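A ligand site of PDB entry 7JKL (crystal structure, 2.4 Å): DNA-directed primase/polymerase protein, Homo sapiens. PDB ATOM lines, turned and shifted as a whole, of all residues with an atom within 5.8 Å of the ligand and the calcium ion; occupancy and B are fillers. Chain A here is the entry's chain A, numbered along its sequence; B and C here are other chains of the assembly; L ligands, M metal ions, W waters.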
ATOM      1  N   GLY A  74     -11.431  -3.715  -2.037  1.00  0.00           N
ATOM      2  CA  GLY A  74     -12.813  -3.470  -1.707  1.00  0.00           C
ATOM      3  C   GLY A  74     -13.818  -4.236  -2.512  1.00  0.00           C
ATOM      4  O   GLY A  74     -15.013  -3.925  -2.467  1.00  0.00           O
ATOM      5  N   ARG A  76     -16.660  -6.378  -3.605  1.00  0.00           N
ATOM      6  CA  ARG A  76     -17.837  -6.656  -2.789  1.00  0.00           C
ATOM      7  C   ARG A  76     -18.813  -7.548  -3.541  1.00  0.00           C
ATOM      8  O   ARG A  76     -18.911  -7.504  -4.772  1.00  0.00           O
ATOM      9  CB  ARG A  76     -18.546  -5.358  -2.377  1.00  0.00           C
ATOM     10  CG  ARG A  76     -17.906  -4.628  -1.211  1.00  0.00           C
ATOM     11  CD  ARG A  76     -18.218  -3.150  -1.251  1.00  0.00           C
ATOM     12  NE  ARG A  76     -17.961  -2.484   0.022  1.00  0.00           N
ATOM     13  CZ  ARG A  76     -16.743  -2.209   0.496  1.00  0.00           C
ATOM     14  NH1 ARG A  76     -15.666  -2.554  -0.190  1.00  0.00           N
ATOM     15  NH2 ARG A  76     -16.613  -1.599   1.666  1.00  0.00           N
ATOM     16  N   TYR A 100     -21.619  -4.615   5.203  1.00  0.00           N
ATOM     17  CA  TYR A 100     -21.930  -3.200   5.068  1.00  0.00           C
ATOM     18  C   TYR A 100     -23.398  -3.036   4.679  1.00  0.00           C
ATOM     19  O   TYR A 100     -23.963  -3.873   3.962  1.00  0.00           O
ATOM     20  CB  TYR A 100     -21.038  -2.522   4.009  1.00  0.00           C
ATOM     21  CG  TYR A 100     -19.570  -2.565   4.342  1.00  0.00           C
ATOM     22  CD1 TYR A 100     -18.797  -3.686   4.048  1.00  0.00           C
ATOM     23  CD2 TYR A 100     -18.940  -1.482   4.944  1.00  0.00           C
ATOM     24  CE1 TYR A 100     -17.453  -3.731   4.352  1.00  0.00           C
ATOM     25  CE2 TYR A 100     -17.590  -1.513   5.247  1.00  0.00           C
ATOM     26  CZ  TYR A 100     -16.852  -2.643   4.955  1.00  0.00           C
ATOM     27  OH  TYR A 100     -15.511  -2.679   5.254  1.00  0.00           O
ATOM     28  N   ASP A 114     -19.986   9.994  10.184  1.00  0.00           N
ATOM     29  CA  ASP A 114     -18.755   9.199  10.180  1.00  0.00           C
ATOM     30  C   ASP A 114     -17.652  10.087  10.757  1.00  0.00           C
ATOM     31  O   ASP A 114     -17.183  11.009  10.085  1.00  0.00           O
ATOM     32  CB  ASP A 114     -18.400   8.714   8.777  1.00  0.00           C
ATOM     33  CG  ASP A 114     -17.175   7.829   8.761  1.00  0.00           C
ATOM     34  OD1 ASP A 114     -17.275   6.659   9.214  1.00  0.00           O
ATOM     35  OD2 ASP A 114     -16.114   8.280   8.292  1.00  0.00           O
ATOM     36  N   LEU A 115     -17.274   9.815  11.995  1.00  0.00           N
ATOM     37  CA  LEU A 115     -16.308  10.635  12.725  1.00  0.00           C
ATOM     38  C   LEU A 115     -14.997   9.886  12.872  1.00  0.00           C
ATOM     39  O   LEU A 115     -14.979   8.693  13.188  1.00  0.00           O
ATOM     40  CB  LEU A 115     -16.867  11.006  14.104  1.00  0.00           C
ATOM     41  CG  LEU A 115     -18.273  11.622  14.101  1.00  0.00           C
ATOM     42  CD1 LEU A 115     -18.744  11.895  15.516  1.00  0.00           C
ATOM     43  CD2 LEU A 115     -18.305  12.901  13.271  1.00  0.00           C
ATOM     44  N   GLU A 116     -13.885  10.597  12.639  1.00  0.00           N
ATOM     45  CA  GLU A 116     -12.580   9.955  12.665  1.00  0.00           C
ATOM     46  C   GLU A 116     -11.483  11.008  12.589  1.00  0.00           C
ATOM     47  O   GLU A 116     -11.583  11.963  11.821  1.00  0.00           O
ATOM     48  CB  GLU A 116     -12.439   8.960  11.499  1.00  0.00           C
ATOM     49  CG  GLU A 116     -12.660   9.585  10.126  1.00  0.00           C
ATOM     50  CD  GLU A 116     -12.739   8.547   9.028  1.00  0.00           C
ATOM     51  OE1 GLU A 116     -12.800   8.937   7.835  1.00  0.00           O
ATOM     52  OE2 GLU A 116     -12.751   7.344   9.338  1.00  0.00           O
ATOM     53  N   SER A 160     -15.383   2.180  16.732  1.00  0.00           N
ATOM     54  CA  SER A 160     -14.507   1.244  16.047  1.00  0.00           C
ATOM     55  C   SER A 160     -13.056   1.710  16.122  1.00  0.00           C
ATOM     56  O   SER A 160     -12.278   1.509  15.180  1.00  0.00           O
ATOM     57  CB  SER A 160     -14.925   1.073  14.579  1.00  0.00           C
ATOM     58  OG  SER A 160     -14.091   0.147  13.910  1.00  0.00           O
ATOM     59  N   SER A 161     -12.680   2.336  17.225  1.00  0.00           N
ATOM     60  CA  SER A 161     -11.389   3.003  17.356  1.00  0.00           C
ATOM     61  C   SER A 161     -10.257   1.985  17.525  1.00  0.00           C
ATOM     62  O   SER A 161     -10.462   0.835  17.917  1.00  0.00           O
ATOM     63  CB  SER A 161     -11.390   3.961  18.538  1.00  0.00           C
ATOM     64  OG  SER A 161     -12.414   4.942  18.399  1.00  0.00           O
ATOM     65  N   LYS A 165      -6.487   5.487  15.512  1.00  0.00           N
ATOM     66  CA  LYS A 165      -7.640   6.150  14.902  1.00  0.00           C
ATOM     67  C   LYS A 165      -8.819   6.138  15.859  1.00  0.00           C
ATOM     68  O   LYS A 165      -9.227   5.078  16.338  1.00  0.00           O
ATOM     69  CB  LYS A 165      -8.022   5.460  13.579  1.00  0.00           C
ATOM     70  CG  LYS A 165      -9.060   6.231  12.771  1.00  0.00           C
ATOM     71  CD  LYS A 165      -9.323   5.551  11.432  1.00  0.00           C
ATOM     72  CE  LYS A 165     -10.341   6.320  10.612  1.00  0.00           C
ATOM     73  NZ  LYS A 165     -10.588   5.695   9.279  1.00  0.00           N
ATOM     74  N   SER A 167     -12.368   6.301  15.833  1.00  0.00           N
ATOM     75  CA  SER A 167     -13.416   6.087  14.839  1.00  0.00           C
ATOM     76  C   SER A 167     -14.746   5.888  15.549  1.00  0.00           C
ATOM     77  O   SER A 167     -14.896   4.978  16.370  1.00  0.00           O
ATOM     78  CB  SER A 167     -13.089   4.896  13.951  1.00  0.00           C
ATOM     79  OG  SER A 167     -14.068   4.737  12.938  1.00  0.00           O
ATOM     80  N   HIS A 169     -19.185   6.107  14.858  1.00  0.00           N
ATOM     81  CA  HIS A 169     -20.370   6.271  14.018  1.00  0.00           C
ATOM     82  C   HIS A 169     -21.536   6.728  14.885  1.00  0.00           C
ATOM     83  O   HIS A 169     -21.813   6.117  15.923  1.00  0.00           O
ATOM     84  CB  HIS A 169     -20.735   4.972  13.303  1.00  0.00           C
ATOM     85  CG  HIS A 169     -19.879   4.648  12.124  1.00  0.00           C
ATOM     86  ND1 HIS A 169     -20.132   3.598  11.277  1.00  0.00           N
ATOM     87  CD2 HIS A 169     -18.759   5.251  11.647  1.00  0.00           C
ATOM     88  CE1 HIS A 169     -19.222   3.556  10.328  1.00  0.00           C
ATOM     89  NE2 HIS A 169     -18.376   4.553  10.524  1.00  0.00           N
ATOM     90  N   ASP A 280     -16.545  13.416   8.562  1.00  0.00           N
ATOM     91  CA  ASP A 280     -16.289  12.944   7.208  1.00  0.00           C
ATOM     92  C   ASP A 280     -17.515  13.218   6.351  1.00  0.00           C
ATOM     93  O   ASP A 280     -18.569  12.588   6.535  1.00  0.00           O
ATOM     94  CB  ASP A 280     -15.932  11.461   7.219  1.00  0.00           C
ATOM     95  CG  ASP A 280     -15.662  10.913   5.826  1.00  0.00           C
ATOM     96  OD1 ASP A 280     -15.634  11.710   4.858  1.00  0.00           O
ATOM     97  OD2 ASP A 280     -15.495   9.677   5.695  1.00  0.00           O
ATOM     98  N   VAL A 283     -19.327  10.385   3.058  1.00  0.00           N
ATOM     99  CA  VAL A 283     -20.155   9.196   3.206  1.00  0.00           C
ATOM    100  C   VAL A 283     -21.612   9.471   2.800  1.00  0.00           C
ATOM    101  O   VAL A 283     -22.511   8.725   3.169  1.00  0.00           O
ATOM    102  CB  VAL A 283     -20.090   8.648   4.642  1.00  0.00           C
ATOM    103  CG1 VAL A 283     -18.662   8.277   4.994  1.00  0.00           C
ATOM    104  CG2 VAL A 283     -20.662   9.670   5.636  1.00  0.00           C
ATOM    105  N   ARG A 288     -24.218   4.385  -0.823  1.00  0.00           N
ATOM    106  CA  ARG A 288     -23.075   4.387   0.083  1.00  0.00           C
ATOM    107  C   ARG A 288     -23.088   3.144   0.957  1.00  0.00           C
ATOM    108  O   ARG A 288     -24.086   2.840   1.619  1.00  0.00           O
ATOM    109  CB  ARG A 288     -23.086   5.651   0.953  1.00  0.00           C
ATOM    110  CG  ARG A 288     -22.116   5.617   2.131  1.00  0.00           C
ATOM    111  CD  ARG A 288     -20.674   5.445   1.691  1.00  0.00           C
ATOM    112  NE  ARG A 288     -20.237   6.514   0.812  1.00  0.00           N
ATOM    113  CZ  ARG A 288     -18.995   6.649   0.344  1.00  0.00           C
ATOM    114  NH1 ARG A 288     -18.064   5.774   0.676  1.00  0.00           N
ATOM    115  NH2 ARG A 288     -18.693   7.671  -0.452  1.00  0.00           N
ATOM    116  N   ASN A 289     -21.967   2.419   0.962  1.00  0.00           N
ATOM    117  CA  ASN A 289     -21.756   1.351   1.920  1.00  0.00           C
ATOM    118  C   ASN A 289     -21.467   1.952   3.294  1.00  0.00           C
ATOM    119  O   ASN A 289     -20.849   3.006   3.425  1.00  0.00           O
ATOM    120  CB  ASN A 289     -20.579   0.469   1.486  1.00  0.00           C
ATOM    121  CG  ASN A 289     -20.930  -0.454   0.322  1.00  0.00           C
ATOM    122  OD1 ASN A 289     -20.696  -1.653   0.375  1.00  0.00           O
ATOM    123  ND2 ASN A 289     -21.489   0.114  -0.740  1.00  0.00           N
ATOM    124  N   PHE A 290     -21.930   1.259   4.335  1.00  0.00           N
ATOM    125  CA  PHE A 290     -21.718   1.723   5.711  1.00  0.00           C
ATOM    126  C   PHE A 290     -21.604   0.503   6.608  1.00  0.00           C
ATOM    127  O   PHE A 290     -22.546  -0.284   6.710  1.00  0.00           O
ATOM    128  CB  PHE A 290     -22.869   2.641   6.152  1.00  0.00           C
ATOM    129  CG  PHE A 290     -22.473   3.679   7.166  1.00  0.00           C
ATOM    130  CD1 PHE A 290     -21.511   4.630   6.864  1.00  0.00           C
ATOM    131  CD2 PHE A 290     -23.071   3.718   8.408  1.00  0.00           C
ATOM    132  CE1 PHE A 290     -21.147   5.589   7.789  1.00  0.00           C
ATOM    133  CE2 PHE A 290     -22.713   4.679   9.341  1.00  0.00           C
ATOM    134  CZ  PHE A 290     -21.751   5.614   9.031  1.00  0.00           C
ATOM    135  N   ARG A 291     -20.444   0.353   7.253  1.00  0.00           N
ATOM    136  CA  ARG A 291     -20.147  -0.856   8.000  1.00  0.00           C
ATOM    137  C   ARG A 291     -21.219  -1.127   9.052  1.00  0.00           C
ATOM    138  O   ARG A 291     -21.607  -0.229   9.800  1.00  0.00           O
ATOM    139  CB  ARG A 291     -18.764  -0.747   8.647  1.00  0.00           C
ATOM    140  CG  ARG A 291     -18.302  -2.021   9.347  1.00  0.00           C
ATOM    141  CD  ARG A 291     -16.785  -2.186   9.288  1.00  0.00           C
ATOM    142  NE  ARG A 291     -16.073  -0.995   9.771  1.00  0.00           N
ATOM    143  CZ  ARG A 291     -15.657  -0.805  11.021  1.00  0.00           C
ATOM    144  NH1 ARG A 291     -15.880  -1.726  11.960  1.00  0.00           N
ATOM    145  NH2 ARG A 291     -15.025   0.309  11.338  1.00  0.00           N
ATOM    146  N   LYS A 297     -13.685  -4.060   9.166  1.00  0.00           N
ATOM    147  CA  LYS A 297     -13.099  -4.103   7.837  1.00  0.00           C
ATOM    148  C   LYS A 297     -12.357  -5.424   7.642  1.00  0.00           C
ATOM    149  O   LYS A 297     -11.823  -6.015   8.589  1.00  0.00           O
ATOM    150  CB  LYS A 297     -12.136  -2.935   7.630  1.00  0.00           C
ATOM    151  CG  LYS A 297     -12.818  -1.576   7.569  1.00  0.00           C
ATOM    152  CD  LYS A 297     -11.873  -0.516   7.006  1.00  0.00           C
ATOM    153  CE  LYS A 297     -12.480   0.876   7.096  1.00  0.00           C
ATOM    154  NZ  LYS A 297     -11.615   1.907   6.455  1.00  0.00           N
ATOM    155  N   LEU A 304     -17.501  -2.593  15.014  1.00  0.00           N
ATOM    156  CA  LEU A 304     -18.288  -1.505  15.571  1.00  0.00           C
ATOM    157  C   LEU A 304     -19.084  -1.998  16.770  1.00  0.00           C
ATOM    158  O   LEU A 304     -19.759  -3.027  16.691  1.00  0.00           O
ATOM    159  CB  LEU A 304     -19.216  -0.918  14.505  1.00  0.00           C
ATOM    160  CG  LEU A 304     -18.564   0.073  13.531  1.00  0.00           C
ATOM    161  CD1 LEU A 304     -19.361   0.161  12.244  1.00  0.00           C
ATOM    162  CD2 LEU A 304     -18.455   1.449  14.166  1.00  0.00           C
ATOM    163  P   8OG B   3     -15.115  -5.946  -9.526  1.00  0.00           P
ATOM    164  OP1 8OG B   3     -14.308  -4.931 -10.298  1.00  0.00           O
ATOM    165  OP2 8OG B   3     -14.217  -6.984  -8.902  1.00  0.00           O
ATOM    166  O5' 8OG B   3     -16.048  -5.205  -8.383  1.00  0.00           O
ATOM    167  C5' 8OG B   3     -16.975  -5.985  -7.682  1.00  0.00           C
ATOM    168  C4' 8OG B   3     -18.179  -5.161  -7.301  1.00  0.00           C
ATOM    169  O4' 8OG B   3     -17.885  -4.355  -5.917  1.00  0.00           O
ATOM    170  C3' 8OG B   3     -18.451  -4.274  -8.217  1.00  0.00           C
ATOM    171  O3' 8OG B   3     -19.929  -4.153  -8.362  1.00  0.00           O
ATOM    172  C2' 8OG B   3     -17.842  -2.945  -7.691  1.00  0.00           C
ATOM    173  C1' 8OG B   3     -17.992  -3.076  -6.162  1.00  0.00           C
ATOM    174  N9  8OG B   3     -16.921  -2.341  -5.465  1.00  0.00           N
ATOM    175  C8  8OG B   3     -17.094  -1.258  -4.421  1.00  0.00           C
ATOM    176  N7  8OG B   3     -15.710  -0.840  -4.000  1.00  0.00           N
ATOM    177  C5  8OG B   3     -14.787  -1.636  -4.751  1.00  0.00           C
ATOM    178  C6  8OG B   3     -13.266  -1.640  -4.732  1.00  0.00           C
ATOM    179  O6  8OG B   3     -12.681  -0.904  -4.016  1.00  0.00           O
ATOM    180  N1  8OG B   3     -12.546  -2.553  -5.598  1.00  0.00           N
ATOM    181  C2  8OG B   3     -13.295  -3.461  -6.484  1.00  0.00           C
ATOM    182  N2  8OG B   3     -12.574  -4.373  -7.351  1.00  0.00           N
ATOM    183  N3  8OG B   3     -14.763  -3.449  -6.492  1.00  0.00           N
ATOM    184  C4  8OG B   3     -15.503  -2.535  -5.615  1.00  0.00           C
ATOM    185  O8  8OG B   3     -18.125  -0.823  -4.018  1.00  0.00           O
ATOM    186  P    DC B   4     -20.559  -3.203  -9.483  1.00  0.00           P
ATOM    187  OP1  DC B   4     -21.924  -3.695  -9.772  1.00  0.00           O
ATOM    188  OP2  DC B   4     -19.582  -3.077 -10.584  1.00  0.00           O
ATOM    189  O5'  DC B   4     -20.677  -1.782  -8.765  1.00  0.00           O
ATOM    190  C5'  DC B   4     -21.523  -1.640  -7.645  1.00  0.00           C
ATOM    191  C4'  DC B   4     -21.377  -0.265  -7.008  1.00  0.00           C
ATOM    192  O4'  DC B   4     -20.028  -0.114  -6.480  1.00  0.00           O
ATOM    193  C3'  DC B   4     -21.595   0.921  -7.961  1.00  0.00           C
ATOM    194  O3'  DC B   4     -22.594   1.799  -7.428  1.00  0.00           O
ATOM    195  C2'  DC B   4     -20.213   1.575  -8.044  1.00  0.00           C
ATOM    196  C1'  DC B   4     -19.635   1.221  -6.688  1.00  0.00           C
ATOM    197  N1   DC B   4     -18.140   1.323  -6.595  1.00  0.00           N
ATOM    198  C2   DC B   4     -17.573   2.112  -5.584  1.00  0.00           C
ATOM    199  O2   DC B   4     -18.310   2.714  -4.805  1.00  0.00           O
ATOM    200  N3   DC B   4     -16.217   2.195  -5.499  1.00  0.00           N
ATOM    201  C4   DC B   4     -15.457   1.535  -6.372  1.00  0.00           C
ATOM    202  N4   DC B   4     -14.131   1.648  -6.242  1.00  0.00           N
ATOM    203  C5   DC B   4     -16.018   0.728  -7.398  1.00  0.00           C
ATOM    204  C6   DC B   4     -17.351   0.642  -7.477  1.00  0.00           C
ATOM    205  P   DDG C  13     -10.438   9.346   3.010  1.00  0.00           P
ATOM    206  OP1 DDG C  13     -10.755  10.473   3.968  1.00  0.00           O
ATOM    207  OP2 DDG C  13      -9.816   8.190   3.765  1.00  0.00           O
ATOM    208  O5' DDG C  13     -11.831   8.840   2.286  1.00  0.00           O
ATOM    209  C5' DDG C  13     -13.025   9.525   2.540  1.00  0.00           C
ATOM    210  C4' DDG C  13     -14.224   8.577   2.239  1.00  0.00           C
ATOM    211  O4' DDG C  13     -14.025   7.906   0.847  1.00  0.00           O
ATOM    212  C3' DDG C  13     -14.292   7.618   3.101  1.00  0.00           C
ATOM    213  C2' DDG C  13     -13.885   6.280   2.313  1.00  0.00           C
ATOM    214  C1' DDG C  13     -14.390   6.468   1.111  1.00  0.00           C
ATOM    215  N9  DDG C  13     -13.878   5.555   0.045  1.00  0.00           N
ATOM    216  C8  DDG C  13     -12.578   5.199   0.019  1.00  0.00           C
ATOM    217  N7  DDG C  13     -12.389   4.371  -1.038  1.00  0.00           N
ATOM    218  C5  DDG C  13     -13.563   4.227  -1.656  1.00  0.00           C
ATOM    219  C6  DDG C  13     -13.991   3.420  -2.893  1.00  0.00           C
ATOM    220  O6  DDG C  13     -13.190   2.787  -3.482  1.00  0.00           O
ATOM    221  N1  DDG C  13     -15.349   3.444  -3.332  1.00  0.00           N
ATOM    222  C2  DDG C  13     -16.319   4.230  -2.600  1.00  0.00           C
ATOM    223  N2  DDG C  13     -17.700   4.279  -3.025  1.00  0.00           N
ATOM    224  N3  DDG C  13     -15.909   4.997  -1.427  1.00  0.00           N
ATOM    225  C4  DDG C  13     -14.487   4.961  -0.975  1.00  0.00           C
HETATM  226  P1  LIG L   1     -12.916   3.202  10.108  1.00  0.00           P
HETATM  227  O1  LIG L   1     -11.650   2.838   9.468  1.00  0.00           O
HETATM  228  O2  LIG L   1     -13.201   4.687   9.876  1.00  0.00           O
HETATM  229  O3  LIG L   1     -12.836   2.925  11.604  1.00  0.00           O
HETATM  230  P2  LIG L   1     -15.353   2.907   8.518  1.00  0.00           P
HETATM  231  O4  LIG L   1     -16.585   2.098   8.653  1.00  0.00           O
HETATM  232  O5  LIG L   1     -15.599   4.260   8.940  1.00  0.00           O
HETATM  233  O6  LIG L   1     -14.177   2.279   9.436  1.00  0.00           O
HETATM  234  P3  LIG L   1     -14.323   4.280   6.128  1.00  0.00           P
HETATM  235  O7  LIG L   1     -12.966   3.953   5.428  1.00  0.00           O
HETATM  236  O8  LIG L   1     -14.133   5.399   7.151  1.00  0.00           O
HETATM  237  O9  LIG L   1     -14.889   2.901   6.912  1.00  0.00           O
HETATM  238  O10 LIG L   1     -15.415   4.751   5.016  1.00  0.00           O
HETATM  239  C1  LIG L   1     -16.729   4.891   5.422  1.00  0.00           C
HETATM  240  C2  LIG L   1     -17.624   4.068   4.525  1.00  0.00           C
HETATM  241  O11 LIG L   1     -17.327   4.275   3.318  1.00  0.00           O
HETATM  242  C3  LIG L   1     -17.382   2.440   4.774  1.00  0.00           C
HETATM  243  O12 LIG L   1     -18.163   1.979   5.960  1.00  0.00           O
HETATM  244  C4  LIG L   1     -17.793   1.900   3.757  1.00  0.00           C
HETATM  245  C5  LIG L   1     -17.425   2.924   2.617  1.00  0.00           C
HETATM  246  N1  LIG L   1     -16.269   2.594   2.091  1.00  0.00           N
HETATM  247  C6  LIG L   1     -14.994   2.751   2.494  1.00  0.00           C
HETATM  248  N2  LIG L   1     -14.195   2.219   1.580  1.00  0.00           N
HETATM  249  C7  LIG L   1     -14.961   1.740   0.608  1.00  0.00           C
HETATM  250  C8  LIG L   1     -14.649   1.086  -0.572  1.00  0.00           C
HETATM  251  N3  LIG L   1     -13.319   0.728  -1.125  1.00  0.00           N
HETATM  252  N4  LIG L   1     -15.616   0.704  -1.379  1.00  0.00           N
HETATM  253  C9  LIG L   1     -16.920   0.938  -1.063  1.00  0.00           C
HETATM  254  N5  LIG L   1     -17.220   1.570   0.094  1.00  0.00           N
HETATM  255  C10 LIG L   1     -16.249   1.967   0.925  1.00  0.00           C
HETATM  256 CA    CA M   1     -14.866   6.335   9.126  1.00  0.00          CA
HETATM  257  O   HOH W   1     -15.055   6.562  11.404  1.00  0.00           O
HETATM  258  O   HOH W   2     -19.784   3.137  -0.781  1.00  0.00           O
HETATM  259  O   HOH W   3     -11.296   1.298  12.577  1.00  0.00           O
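Merely in contact with the ligand: Asn 289, Phe 290, Tyr 100, Ser 160 and Val 283.
Hydrophobic or aromatic side chains that line the ligand: Tyr 100, His 169 and Val 283.
Within 4 Å of the ligand: Arg 76, Tyr 100, Asp 114, Glu 116, Ser 160, Lys 165, Ser 167, His 169, Val 283, Arg 288, Asn 289, Phe 290, Arg 291, Lys 297, 8OG 3 of chain B and DDG 13 of chain C.
OE2 of Glu 116 lies close to NZ of Lys 165.
The side-chain carboxylate (OD1) of Asp 114 lies close to a ring nitrogen (NE2) of His 169, 2.7 Å away.
The backbone carbonyl oxygen (O) of Asp 114 sits at hydrogen-bond distance from the backbone NH (N) of Asp 280, at 2.9 Å.
The backbone NH (N) of Ser 160 sits at hydrogen-bond distance from the backbone carbonyl oxygen (O) of Ser 167, 2.9 Å away.
O4' of 8OG 3 of chain B sits at hydrogen-bond distance from the backbone NH (N) of Arg 76 (3.3 Å).
N3 of DDG 13 of chain C lies within hydrogen-bond range of the guanidinium group of Arg 288, at 3.1 Å.
OD1 of Asn 289 sits at hydrogen-bond distance from NE of Arg 76, 2.9 Å away.
NH1 of Arg 76 is in hydrogen-bond range of O of Gly 74 (2.7 Å).
Water W1 bridges OG of Ser 167 (2.6 Å) and O of Leu 115 (2.8 Å).
Water W3 bridges O3 of the ligand (2.4 Å) and O of Ser 160 (2.8 Å).
Water W2 lies within hydrogen-bond range of the backbone NH (N) of Asn 289 (2.9 Å), a nitrogen (N5) of the ligand (3.1 Å), N2 of DDG 13 of chain C (3.3 Å) and the guanidinium group (NH1) of Arg 288 (3.5 Å).
The side-chain hydroxyl (OG) of Ser 167 sits at hydrogen-bond distance from an oxygen (O3) of the ligand, 2.6 Å away.
An oxygen (O7) of the ligand is in salt-bridge range of the side-chain amino group (NZ) of Lys 297 (2.7 Å).
An oxygen (O1) of the ligand lies within salt-bridge range of the side-chain amino group (NZ) of Lys 165 (3.1 Å).
The backbone NH (N) of Arg 291 lies within hydrogen-bond range of an oxygen (O12) of the ligand, 3.1 Å away.
An oxygen (O4) of the ligand lies within salt-bridge range of the guanidinium group (NE) of Arg 291, 3.3 Å away.
O6 of 8OG 3 of chain B is in hydrogen-bond range of N3 of the ligand, 3.4 Å away.
NH1 of Arg 288 lies within hydrogen-bond range of O11 of the ligand (3.1 Å).
O6 of DDG 13 of chain C sits at hydrogen-bond distance from N3 of the ligand (3.1 Å).
An oxygen (O5) of the ligand sits close to a ring nitrogen (NE2) of His 169, at 3.2 Å.
NH1 of Arg 76 is in hydrogen-bond range of N4 of the ligand (3.5 Å).
An oxygen (O5) of the ligand is bound to the calcium ion (2.2 Å).
Water W1 is bound to the calcium ion, 2.3 Å away.
O8 of the ligand is bound to the calcium ion.
The side-chain carboxylate (OE2) of Glu 116 is bound to the calcium ion (2.4 Å).
The calcium ion is bound by OD1 of Asp 114, at 2.4 Å.
The side-chain carboxylate (OD2) of Asp 114 is bound to the calcium ion.
An oxygen (O2) of the ligand is bound to the calcium ion (2.5 Å).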
